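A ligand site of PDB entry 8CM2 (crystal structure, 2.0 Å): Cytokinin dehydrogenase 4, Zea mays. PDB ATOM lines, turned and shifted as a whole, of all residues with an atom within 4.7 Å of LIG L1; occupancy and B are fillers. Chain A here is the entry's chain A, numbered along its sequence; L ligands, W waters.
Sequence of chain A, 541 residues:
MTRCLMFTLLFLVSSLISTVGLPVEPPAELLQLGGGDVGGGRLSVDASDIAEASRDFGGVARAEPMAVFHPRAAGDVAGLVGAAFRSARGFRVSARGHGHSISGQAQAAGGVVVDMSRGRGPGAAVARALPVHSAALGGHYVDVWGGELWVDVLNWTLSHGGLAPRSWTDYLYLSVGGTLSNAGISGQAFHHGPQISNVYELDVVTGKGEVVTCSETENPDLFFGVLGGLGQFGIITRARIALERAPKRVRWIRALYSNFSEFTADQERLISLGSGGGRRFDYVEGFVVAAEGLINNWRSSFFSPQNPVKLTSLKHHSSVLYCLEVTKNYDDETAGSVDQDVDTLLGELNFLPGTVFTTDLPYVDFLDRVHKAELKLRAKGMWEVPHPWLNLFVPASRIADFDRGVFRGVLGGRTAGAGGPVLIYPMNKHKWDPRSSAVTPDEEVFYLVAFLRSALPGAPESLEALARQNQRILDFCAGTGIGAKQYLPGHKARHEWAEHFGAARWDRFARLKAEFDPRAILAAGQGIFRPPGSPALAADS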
ATOM      1  N   PHE A  57      -1.489  33.098 -33.639  1.00  0.00           N
ATOM      2  CA  PHE A  57      -0.737  32.584 -32.496  1.00  0.00           C
ATOM      3  C   PHE A  57      -0.108  31.175 -32.740  1.00  0.00           C
ATOM      4  O   PHE A  57       0.888  30.823 -32.084  1.00  0.00           O
ATOM      5  CB  PHE A  57      -1.641  32.618 -31.291  1.00  0.00           C
ATOM      6  CG  PHE A  57      -1.039  32.158 -29.991  1.00  0.00           C
ATOM      7  CD1 PHE A  57      -0.279  33.024 -29.213  1.00  0.00           C
ATOM      8  CD2 PHE A  57      -1.292  30.868 -29.508  1.00  0.00           C
ATOM      9  CE1 PHE A  57       0.216  32.621 -27.966  1.00  0.00           C
ATOM     10  CE2 PHE A  57      -0.823  30.481 -28.257  1.00  0.00           C
ATOM     11  CZ  PHE A  57      -0.062  31.354 -27.498  1.00  0.00           C
ATOM     12  N   ASP A 170      -9.745  31.236 -19.999  1.00  0.00           N
ATOM     13  CA  ASP A 170      -8.598  31.314 -19.084  1.00  0.00           C
ATOM     14  C   ASP A 170      -7.793  32.567 -19.442  1.00  0.00           C
ATOM     15  O   ASP A 170      -7.143  33.139 -18.595  1.00  0.00           O
ATOM     16  CB  ASP A 170      -7.663  30.086 -19.251  1.00  0.00           C
ATOM     17  CG  ASP A 170      -8.178  28.778 -18.656  1.00  0.00           C
ATOM     18  OD1 ASP A 170      -9.183  28.802 -17.929  1.00  0.00           O
ATOM     19  OD2 ASP A 170      -7.555  27.751 -18.915  1.00  0.00           O
ATOM     20  N   ILE A 185     -14.504  28.665 -23.114  1.00  0.00           N
ATOM     21  CA  ILE A 185     -14.424  27.724 -21.993  1.00  0.00           C
ATOM     22  C   ILE A 185     -13.331  28.095 -20.980  1.00  0.00           C
ATOM     23  O   ILE A 185     -12.231  28.502 -21.335  1.00  0.00           O
ATOM     24  CB  ILE A 185     -14.169  26.274 -22.545  1.00  0.00           C
ATOM     25  CG1 ILE A 185     -15.107  25.889 -23.700  1.00  0.00           C
ATOM     26  CG2 ILE A 185     -14.248  25.224 -21.443  1.00  0.00           C
ATOM     27  CD1 ILE A 185     -14.611  24.624 -24.488  1.00  0.00           C
ATOM     28  N   GLU A 285     -10.988  23.396 -12.572  1.00  0.00           N
ATOM     29  CA  GLU A 285     -10.026  23.018 -13.586  1.00  0.00           C
ATOM     30  C   GLU A 285      -9.096  21.952 -12.984  1.00  0.00           C
ATOM     31  O   GLU A 285      -9.368  21.406 -11.900  1.00  0.00           O
ATOM     32  CB  GLU A 285      -9.253  24.191 -14.198  1.00  0.00           C
ATOM     33  CG  GLU A 285     -10.127  25.034 -15.097  1.00  0.00           C
ATOM     34  CD  GLU A 285      -9.399  25.978 -16.005  1.00  0.00           C
ATOM     35  OE1 GLU A 285     -10.054  26.880 -16.568  1.00  0.00           O
ATOM     36  OE2 GLU A 285      -8.153  25.852 -16.142  1.00  0.00           O
ATOM     37  N   VAL A 370      -3.338  34.502 -16.628  1.00  0.00           N
ATOM     38  CA  VAL A 370      -2.648  33.957 -17.807  1.00  0.00           C
ATOM     39  C   VAL A 370      -1.909  35.073 -18.568  1.00  0.00           C
ATOM     40  O   VAL A 370      -0.866  34.824 -19.201  1.00  0.00           O
ATOM     41  CB  VAL A 370      -3.610  33.087 -18.676  1.00  0.00           C
ATOM     42  CG1 VAL A 370      -2.929  32.620 -19.966  1.00  0.00           C
ATOM     43  CG2 VAL A 370      -4.139  31.884 -17.865  1.00  0.00           C
ATOM     44  N   ALA A 373       1.442  35.262 -16.921  1.00  0.00           N
ATOM     45  CA  ALA A 373       2.278  34.182 -17.437  1.00  0.00           C
ATOM     46  C   ALA A 373       2.795  34.632 -18.811  1.00  0.00           C
ATOM     47  O   ALA A 373       3.991  34.434 -19.095  1.00  0.00           O
ATOM     48  CB  ALA A 373       1.463  32.901 -17.546  1.00  0.00           C
ATOM     49  N   GLU A 374       1.936  35.299 -19.622  1.00  0.00           N
ATOM     50  CA  GLU A 374       2.318  35.855 -20.927  1.00  0.00           C
ATOM     51  C   GLU A 374       3.483  36.858 -20.813  1.00  0.00           C
ATOM     52  O   GLU A 374       4.391  36.820 -21.648  1.00  0.00           O
ATOM     53  CB  GLU A 374       1.111  36.512 -21.630  1.00  0.00           C
ATOM     54  CG  GLU A 374       1.501  37.439 -22.773  1.00  0.00           C
ATOM     55  CD  GLU A 374       0.399  38.253 -23.413  1.00  0.00           C
ATOM     56  OE1 GLU A 374      -0.759  38.186 -22.943  1.00  0.00           O
ATOM     57  OE2 GLU A 374       0.689  38.955 -24.409  1.00  0.00           O
ATOM     58  N   LEU A 377       6.826  35.176 -20.312  1.00  0.00           N
ATOM     59  CA  LEU A 377       7.240  34.543 -21.564  1.00  0.00           C
ATOM     60  C   LEU A 377       7.814  35.529 -22.576  1.00  0.00           C
ATOM     61  O   LEU A 377       8.809  35.217 -23.234  1.00  0.00           O
ATOM     62  CB  LEU A 377       6.084  33.752 -22.209  1.00  0.00           C
ATOM     63  CG  LEU A 377       5.629  32.474 -21.482  1.00  0.00           C
ATOM     64  CD1 LEU A 377       4.252  32.062 -21.937  1.00  0.00           C
ATOM     65  CD2 LEU A 377       6.629  31.324 -21.669  1.00  0.00           C
ATOM     66  N   TRP A 383       7.399  33.868 -26.242  1.00  0.00           N
ATOM     67  CA  TRP A 383       6.009  34.123 -26.580  1.00  0.00           C
ATOM     68  C   TRP A 383       5.784  34.045 -28.081  1.00  0.00           C
ATOM     69  O   TRP A 383       4.783  33.492 -28.503  1.00  0.00           O
ATOM     70  CB  TRP A 383       5.531  35.480 -26.014  1.00  0.00           C
ATOM     71  CG  TRP A 383       4.127  35.857 -26.396  1.00  0.00           C
ATOM     72  CD1 TRP A 383       3.749  36.707 -27.402  1.00  0.00           C
ATOM     73  CD2 TRP A 383       2.910  35.386 -25.795  1.00  0.00           C
ATOM     74  NE1 TRP A 383       2.372  36.785 -27.461  1.00  0.00           N
ATOM     75  CE2 TRP A 383       1.834  36.014 -26.467  1.00  0.00           C
ATOM     76  CE3 TRP A 383       2.629  34.510 -24.733  1.00  0.00           C
ATOM     77  CZ2 TRP A 383       0.501  35.763 -26.139  1.00  0.00           C
ATOM     78  CZ3 TRP A 383       1.303  34.265 -24.402  1.00  0.00           C
ATOM     79  CH2 TRP A 383       0.257  34.896 -25.092  1.00  0.00           C
ATOM     80  N   TRP A 389      -1.021  23.886 -30.407  1.00  0.00           N
ATOM     81  CA  TRP A 389      -1.960  23.558 -29.342  1.00  0.00           C
ATOM     82  C   TRP A 389      -3.114  22.716 -29.845  1.00  0.00           C
ATOM     83  O   TRP A 389      -3.688  22.985 -30.912  1.00  0.00           O
ATOM     84  CB  TRP A 389      -2.444  24.835 -28.655  1.00  0.00           C
ATOM     85  CG  TRP A 389      -1.376  25.527 -27.840  1.00  0.00           C
ATOM     86  CD1 TRP A 389      -0.066  25.163 -27.705  1.00  0.00           C
ATOM     87  CD2 TRP A 389      -1.547  26.707 -27.035  1.00  0.00           C
ATOM     88  NE1 TRP A 389       0.581  26.009 -26.826  1.00  0.00           N
ATOM     89  CE2 TRP A 389      -0.323  26.952 -26.375  1.00  0.00           C
ATOM     90  CE3 TRP A 389      -2.651  27.549 -26.762  1.00  0.00           C
ATOM     91  CZ2 TRP A 389      -0.144  28.037 -25.491  1.00  0.00           C
ATOM     92  CZ3 TRP A 389      -2.475  28.604 -25.879  1.00  0.00           C
ATOM     93  CH2 TRP A 389      -1.243  28.839 -25.253  1.00  0.00           C
ATOM     94  N   ASN A 391      -6.764  20.827 -28.627  1.00  0.00           N
ATOM     95  CA  ASN A 391      -7.830  20.846 -27.641  1.00  0.00           C
ATOM     96  C   ASN A 391      -8.831  19.758 -27.953  1.00  0.00           C
ATOM     97  O   ASN A 391      -9.422  19.767 -29.027  1.00  0.00           O
ATOM     98  CB  ASN A 391      -8.492  22.263 -27.578  1.00  0.00           C
ATOM     99  CG  ASN A 391      -7.473  23.262 -27.084  1.00  0.00           C
ATOM    100  OD1 ASN A 391      -7.140  23.280 -25.903  1.00  0.00           O
ATOM    101  ND2 ASN A 391      -6.861  24.029 -27.978  1.00  0.00           N
ATOM    102  N   PRO A 421       1.570  23.726 -20.302  1.00  0.00           N
ATOM    103  CA  PRO A 421       0.580  22.949 -19.548  1.00  0.00           C
ATOM    104  C   PRO A 421      -0.288  21.983 -20.359  1.00  0.00           C
ATOM    105  O   PRO A 421      -0.441  22.118 -21.566  1.00  0.00           O
ATOM    106  CB  PRO A 421      -0.258  24.029 -18.841  1.00  0.00           C
ATOM    107  CG  PRO A 421      -0.083  25.256 -19.640  1.00  0.00           C
ATOM    108  CD  PRO A 421       1.159  25.132 -20.478  1.00  0.00           C
ATOM    109  N   LEU A 423      -3.977  20.755 -19.528  1.00  0.00           N
ATOM    110  CA  LEU A 423      -5.113  20.969 -18.628  1.00  0.00           C
ATOM    111  C   LEU A 423      -6.168  19.889 -18.845  1.00  0.00           C
ATOM    112  O   LEU A 423      -6.297  19.358 -19.945  1.00  0.00           O
ATOM    113  CB  LEU A 423      -5.729  22.378 -18.830  1.00  0.00           C
ATOM    114  CG  LEU A 423      -4.810  23.622 -18.746  1.00  0.00           C
ATOM    115  CD1 LEU A 423      -5.624  24.879 -18.496  1.00  0.00           C
ATOM    116  CD2 LEU A 423      -3.840  23.519 -17.601  1.00  0.00           C
ATOM    117  N   TYR A 425     -10.269  18.802 -17.243  1.00  0.00           N
ATOM    118  CA  TYR A 425     -11.417  18.963 -16.341  1.00  0.00           C
ATOM    119  C   TYR A 425     -12.723  18.605 -17.005  1.00  0.00           C
ATOM    120  O   TYR A 425     -12.896  18.833 -18.214  1.00  0.00           O
ATOM    121  CB  TYR A 425     -11.474  20.374 -15.701  1.00  0.00           C
ATOM    122  CG  TYR A 425     -11.419  21.520 -16.687  1.00  0.00           C
ATOM    123  CD1 TYR A 425     -10.197  22.053 -17.105  1.00  0.00           C
ATOM    124  CD2 TYR A 425     -12.584  22.129 -17.139  1.00  0.00           C
ATOM    125  CE1 TYR A 425     -10.145  23.155 -17.947  1.00  0.00           C
ATOM    126  CE2 TYR A 425     -12.532  23.244 -17.975  1.00  0.00           C
ATOM    127  CZ  TYR A 425     -11.319  23.772 -18.354  1.00  0.00           C
ATOM    128  OH  TYR A 425     -11.298  24.850 -19.207  1.00  0.00           O
ATOM    129  N   LEU A 448     -12.544  18.335 -21.114  1.00  0.00           N
ATOM    130  CA  LEU A 448     -11.702  19.063 -22.014  1.00  0.00           C
ATOM    131  C   LEU A 448     -10.290  18.622 -21.622  1.00  0.00           C
ATOM    132  O   LEU A 448      -9.967  18.534 -20.437  1.00  0.00           O
ATOM    133  CB  LEU A 448     -11.839  20.590 -21.850  1.00  0.00           C
ATOM    134  CG  LEU A 448     -10.651  21.455 -22.388  1.00  0.00           C
ATOM    135  CD1 LEU A 448     -10.567  21.451 -23.956  1.00  0.00           C
ATOM    136  CD2 LEU A 448     -10.759  22.873 -21.846  1.00  0.00           C
ATOM    137  N   ALA A 450      -6.637  19.891 -22.813  1.00  0.00           N
ATOM    138  CA  ALA A 450      -5.940  20.958 -23.532  1.00  0.00           C
ATOM    139  C   ALA A 450      -4.419  20.751 -23.485  1.00  0.00           C
ATOM    140  O   ALA A 450      -3.818  20.777 -22.408  1.00  0.00           O
ATOM    141  CB  ALA A 450      -6.333  22.327 -22.933  1.00  0.00           C
ATOM    142  N   LEU A 452      -1.291  22.294 -24.292  1.00  0.00           N
ATOM    143  CA  LEU A 452      -0.821  23.650 -24.566  1.00  0.00           C
ATOM    144  C   LEU A 452       0.687  23.732 -24.567  1.00  0.00           C
ATOM    145  O   LEU A 452       1.300  24.525 -23.847  1.00  0.00           O
ATOM    146  CB  LEU A 452      -1.480  24.645 -23.577  1.00  0.00           C
ATOM    147  CG  LEU A 452      -3.014  24.577 -23.466  1.00  0.00           C
ATOM    148  CD1 LEU A 452      -3.511  25.654 -22.596  1.00  0.00           C
ATOM    149  CD2 LEU A 452      -3.708  24.705 -24.847  1.00  0.00           C
ATOM    150  N   TYR A 487     -11.991  20.630 -30.148  1.00  0.00           N
ATOM    151  CA  TYR A 487     -12.453  21.997 -29.906  1.00  0.00           C
ATOM    152  C   TYR A 487     -11.453  22.844 -30.731  1.00  0.00           C
ATOM    153  O   TYR A 487     -10.268  22.502 -30.779  1.00  0.00           O
ATOM    154  CB  TYR A 487     -12.407  22.357 -28.416  1.00  0.00           C
ATOM    155  CG  TYR A 487     -12.697  23.834 -28.122  1.00  0.00           C
ATOM    156  CD1 TYR A 487     -13.919  24.411 -28.493  1.00  0.00           C
ATOM    157  CD2 TYR A 487     -11.826  24.595 -27.351  1.00  0.00           C
ATOM    158  CE1 TYR A 487     -14.210  25.744 -28.176  1.00  0.00           C
ATOM    159  CE2 TYR A 487     -12.119  25.922 -27.014  1.00  0.00           C
ATOM    160  CZ  TYR A 487     -13.319  26.487 -27.420  1.00  0.00           C
ATOM    161  OH  TYR A 487     -13.586  27.791 -27.068  1.00  0.00           O
ATOM    162  N   LEU A 488     -11.947  23.905 -31.396  1.00  0.00           N
ATOM    163  CA  LEU A 488     -11.187  24.769 -32.362  1.00  0.00           C
ATOM    164  C   LEU A 488     -10.708  23.788 -33.434  1.00  0.00           C
ATOM    165  O   LEU A 488      -9.491  23.634 -33.615  1.00  0.00           O
ATOM    166  CB  LEU A 488     -10.001  25.510 -31.690  1.00  0.00           C
ATOM    167  CG  LEU A 488     -10.228  26.164 -30.309  1.00  0.00           C
ATOM    168  CD1 LEU A 488      -8.925  26.667 -29.733  1.00  0.00           C
ATOM    169  CD2 LEU A 488     -11.216  27.308 -30.399  1.00  0.00           C
HETATM  170  N1  LIG L   1      -3.114  27.492 -16.850  1.00  0.00           N
HETATM  171  C1  LIG L   1      -2.747  28.628 -18.952  1.00  0.00           C
HETATM  172  C2  LIG L   1      -1.420  28.898 -18.636  1.00  0.00           C
HETATM  173  C3  LIG L   1      -0.529  29.358 -19.595  1.00  0.00           C
HETATM  174  C4  LIG L   1      -0.972  29.548 -20.891  1.00  0.00           C
HETATM  175  C5  LIG L   1      -2.288  29.310 -21.238  1.00  0.00           C
HETATM  176  C6  LIG L   1      -6.249  27.614 -24.556  1.00  0.00           C
HETATM  177  C7  LIG L   1      -6.931  27.174 -25.678  1.00  0.00           C
HETATM  178  C8  LIG L   1      -8.665  26.265 -24.327  1.00  0.00           C
HETATM  179  C9  LIG L   1      -8.015  26.692 -23.159  1.00  0.00           C
HETATM  180  C10 LIG L   1      -8.128  25.411 -21.003  1.00  0.00           C
HETATM  181  C11 LIG L   1      -3.668  28.125 -17.883  1.00  0.00           C
HETATM  182  O1  LIG L   1      -4.882  28.319 -17.985  1.00  0.00           O
HETATM  183  O2  LIG L   1      -0.077  29.712 -21.954  1.00  0.00           O
HETATM  184  C12 LIG L   1       0.278  30.928 -22.338  1.00  0.00           C
HETATM  185  F1  LIG L   1      -0.738  31.700 -22.753  1.00  0.00           F
HETATM  186  F2  LIG L   1       1.141  30.858 -23.347  1.00  0.00           F
HETATM  187  F3  LIG L   1       0.889  31.530 -21.335  1.00  0.00           F
HETATM  188  C13 LIG L   1      -3.193  28.839 -20.284  1.00  0.00           C
HETATM  189  N2  LIG L   1      -4.525  28.499 -20.656  1.00  0.00           N
HETATM  190  C14 LIG L   1      -5.015  28.506 -21.936  1.00  0.00           C
HETATM  191  O3  LIG L   1      -4.488  29.111 -22.862  1.00  0.00           O
HETATM  192  N3  LIG L   1      -6.161  27.760 -22.075  1.00  0.00           N
HETATM  193  C15 LIG L   1      -6.791  27.378 -23.290  1.00  0.00           C
HETATM  194 CL1  LIG L   1      -6.260  27.502 -27.253  1.00  0.00          CL
HETATM  195  C16 LIG L   1      -8.137  26.503 -25.594  1.00  0.00           C
HETATM  196 CL2  LIG L   1     -10.156  25.394 -24.187  1.00  0.00          CL
HETATM  197  C17 LIG L   1      -8.699  26.553 -21.816  1.00  0.00           C
HETATM  198  O4  LIG L   1      -8.782  25.403 -19.739  1.00  0.00           O
HETATM  199  P1  LG2 L   2      -9.513  34.799 -34.214  1.00  0.00           P
HETATM  200  O1  LG2 L   2      -8.455  33.809 -33.915  1.00  0.00           O
HETATM  201  O2  LG2 L   2      -8.970  36.058 -34.888  1.00  0.00           O
HETATM  202  O3  LG2 L   2     -10.794  34.252 -35.049  1.00  0.00           O
HETATM  203  C1  LG2 L   2     -11.205  32.871 -34.886  1.00  0.00           C
HETATM  204  C2  LG2 L   2     -12.223  32.510 -35.943  1.00  0.00           C
HETATM  205  O4  LG2 L   2     -13.414  33.310 -35.744  1.00  0.00           O
HETATM  206  C3  LG2 L   2     -11.808  32.752 -37.387  1.00  0.00           C
HETATM  207  O5  LG2 L   2     -12.455  31.835 -38.259  1.00  0.00           O
HETATM  208  C4  LG2 L   2     -12.263  34.202 -37.615  1.00  0.00           C
HETATM  209  O6  LG2 L   2     -12.456  34.593 -38.981  1.00  0.00           O
HETATM  210  C5  LG2 L   2     -13.568  34.229 -36.826  1.00  0.00           C
HETATM  211  N1  LG2 L   2     -13.966  35.525 -36.275  1.00  0.00           N
HETATM  212  C6  LG2 L   2     -13.197  36.396 -35.537  1.00  0.00           C
HETATM  213  N2  LG2 L   2     -13.861  37.403 -35.044  1.00  0.00           N
HETATM  214  C7  LG2 L   2     -15.154  37.204 -35.502  1.00  0.00           C
HETATM  215  C8  LG2 L   2     -16.358  37.929 -35.321  1.00  0.00           C
HETATM  216  N3  LG2 L   2     -16.423  39.102 -34.691  1.00  0.00           N
HETATM  217  N4  LG2 L   2     -17.494  37.410 -35.848  1.00  0.00           N
HETATM  218  C9  LG2 L   2     -17.417  36.263 -36.531  1.00  0.00           C
HETATM  219  N5  LG2 L   2     -16.348  35.507 -36.787  1.00  0.00           N
HETATM  220  C10 LG2 L   2     -15.240  36.039 -36.248  1.00  0.00           C
HETATM  221  N6  LG2 L   2     -10.205  29.495 -25.854  1.00  0.00           N
HETATM  222  C11 LG2 L   2     -11.006  29.111 -24.830  1.00  0.00           C
HETATM  223  O7  LG2 L   2     -12.152  28.719 -25.014  1.00  0.00           O
HETATM  224  N7  LG2 L   2     -10.543  29.200 -23.540  1.00  0.00           N
HETATM  225  C12 LG2 L   2      -9.318  29.690 -23.165  1.00  0.00           C
HETATM  226  O8  LG2 L   2      -8.996  29.673 -21.987  1.00  0.00           O
HETATM  227  C13 LG2 L   2      -8.469  30.107 -24.249  1.00  0.00           C
HETATM  228  N8  LG2 L   2      -7.279  30.565 -23.963  1.00  0.00           N
HETATM  229  C14 LG2 L   2      -6.462  30.944 -25.019  1.00  0.00           C
HETATM  230  C15 LG2 L   2      -5.195  31.458 -24.739  1.00  0.00           C
HETATM  231  C16 LG2 L   2      -4.367  31.917 -25.746  1.00  0.00           C
HETATM  232  C17 LG2 L   2      -2.983  32.416 -25.388  1.00  0.00           C
HETATM  233  C18 LG2 L   2      -4.802  31.875 -27.070  1.00  0.00           C
HETATM  234  C19 LG2 L   2      -3.984  32.466 -28.191  1.00  0.00           C
HETATM  235  C20 LG2 L   2      -6.051  31.327 -27.361  1.00  0.00           C
HETATM  236  C21 LG2 L   2      -6.888  30.858 -26.348  1.00  0.00           C
HETATM  237  N9  LG2 L   2      -8.180  30.317 -26.607  1.00  0.00           N
HETATM  238  C22 LG2 L   2      -8.994  29.947 -25.579  1.00  0.00           C
HETATM  239  C23 LG2 L   2      -8.677  30.127 -27.988  1.00  0.00           C
HETATM  240  C24 LG2 L   2      -9.608  31.213 -28.520  1.00  0.00           C
HETATM  241  O9  LG2 L   2     -10.912  31.072 -27.959  1.00  0.00           O
HETATM  242  C25 LG2 L   2      -9.696  31.142 -30.050  1.00  0.00           C
HETATM  243  O10 LG2 L   2      -8.402  31.414 -30.575  1.00  0.00           O
HETATM  244  C26 LG2 L   2     -10.731  32.020 -30.758  1.00  0.00           C
HETATM  245  O11 LG2 L   2     -10.519  31.947 -32.159  1.00  0.00           O
HETATM  246  C27 LG2 L   2     -10.758  33.455 -30.256  1.00  0.00           C
HETATM  247  O12 LG2 L   2      -9.502  34.112 -30.522  1.00  0.00           O
HETATM  248  P2  LG2 L   2      -9.600  35.510 -31.378  1.00  0.00           P
HETATM  249  O13 LG2 L   2     -10.502  36.482 -30.736  1.00  0.00           O
HETATM  250  O14 LG2 L   2      -8.212  36.090 -31.586  1.00  0.00           O
HETATM  251  O15 LG2 L   2     -10.184  35.192 -32.822  1.00  0.00           O
HETATM  252  O   HOH W   1      -6.497  27.996 -15.961  1.00  0.00           O
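Glu 285 touches LIG L1 (OE2 to O4, 3.7 Å). Val 370 touches LIG L1. CD1 of Leu 377 touches F3 of LIG L1 (3.5 Å). CZ3 of Trp 383 touches F2 of LIG L1 (3.6 Å). CH2 of Trp 389 touches O2 of LIG L1 (3.6 Å). Asn 391 touches LIG L1 (OD1 to C16, 3.4 Å). CD1 of Leu 423 touches O4 of LIG L1, at 3.4 Å. Leu 448 touches LIG L1 (CD2 to CL2, 3.5 Å). CD1 of Leu 452 touches C14 of LIG L1, 3.3 Å away. CE2 of Tyr 487 touches CL2 of LIG L1, at 3.5 Å. Leu 488 touches LIG L1 (CD1 to CL1, 3.7 Å). The nearest printed residue that does not touch LIG L1 is Pro 421 (4.01 Å).
The backbone carbonyl oxygen of Tyr 425 sits at hydrogen-bond distance from the backbone NH of Leu 448 (3.0 Å). NE1 of Trp 389 sits close to O of Leu 452. N of Tyr 487 is in hydrogen-bond range of O of Asn 391 (2.9 Å). The backbone NH (N) of Leu 452 lies within hydrogen-bond range of the backbone carbonyl oxygen (O) of Pro 421 (2.9 Å). The backbone carbonyl oxygen (O) of Ala 450 lies within hydrogen-bond range of the backbone NH (N) of Leu 423. The side-chain carboxylate (OD1) of Asp 170 sits close to the side-chain carboxylate (OE1) of Glu 285.
N3 of LIG L1 sits close to O8 of LG2 L2, 3.4 Å away.
OH of Tyr 487 sits at hydrogen-bond distance from O7 of LG2 L2, 2.7 Å away. The backbone NH of Ile 185 is in hydrogen-bond range of an oxygen (O7) of LG2 L2, at 3.0 Å. The backbone NH of Asp 170 is in hydrogen-bond range of an oxygen (O8) of LG2 L2, 2.6 Å away. The side-chain hydroxyl (OH) of Tyr 425 is in hydrogen-bond range of an oxygen (O4) of LIG L1. O4 of LIG L1 lies within hydrogen-bond range of OD2 of Asp 170, 2.8 Å away. N7 of LG2 L2 lies within hydrogen-bond range of O of Ile 185, at 2.9 Å.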
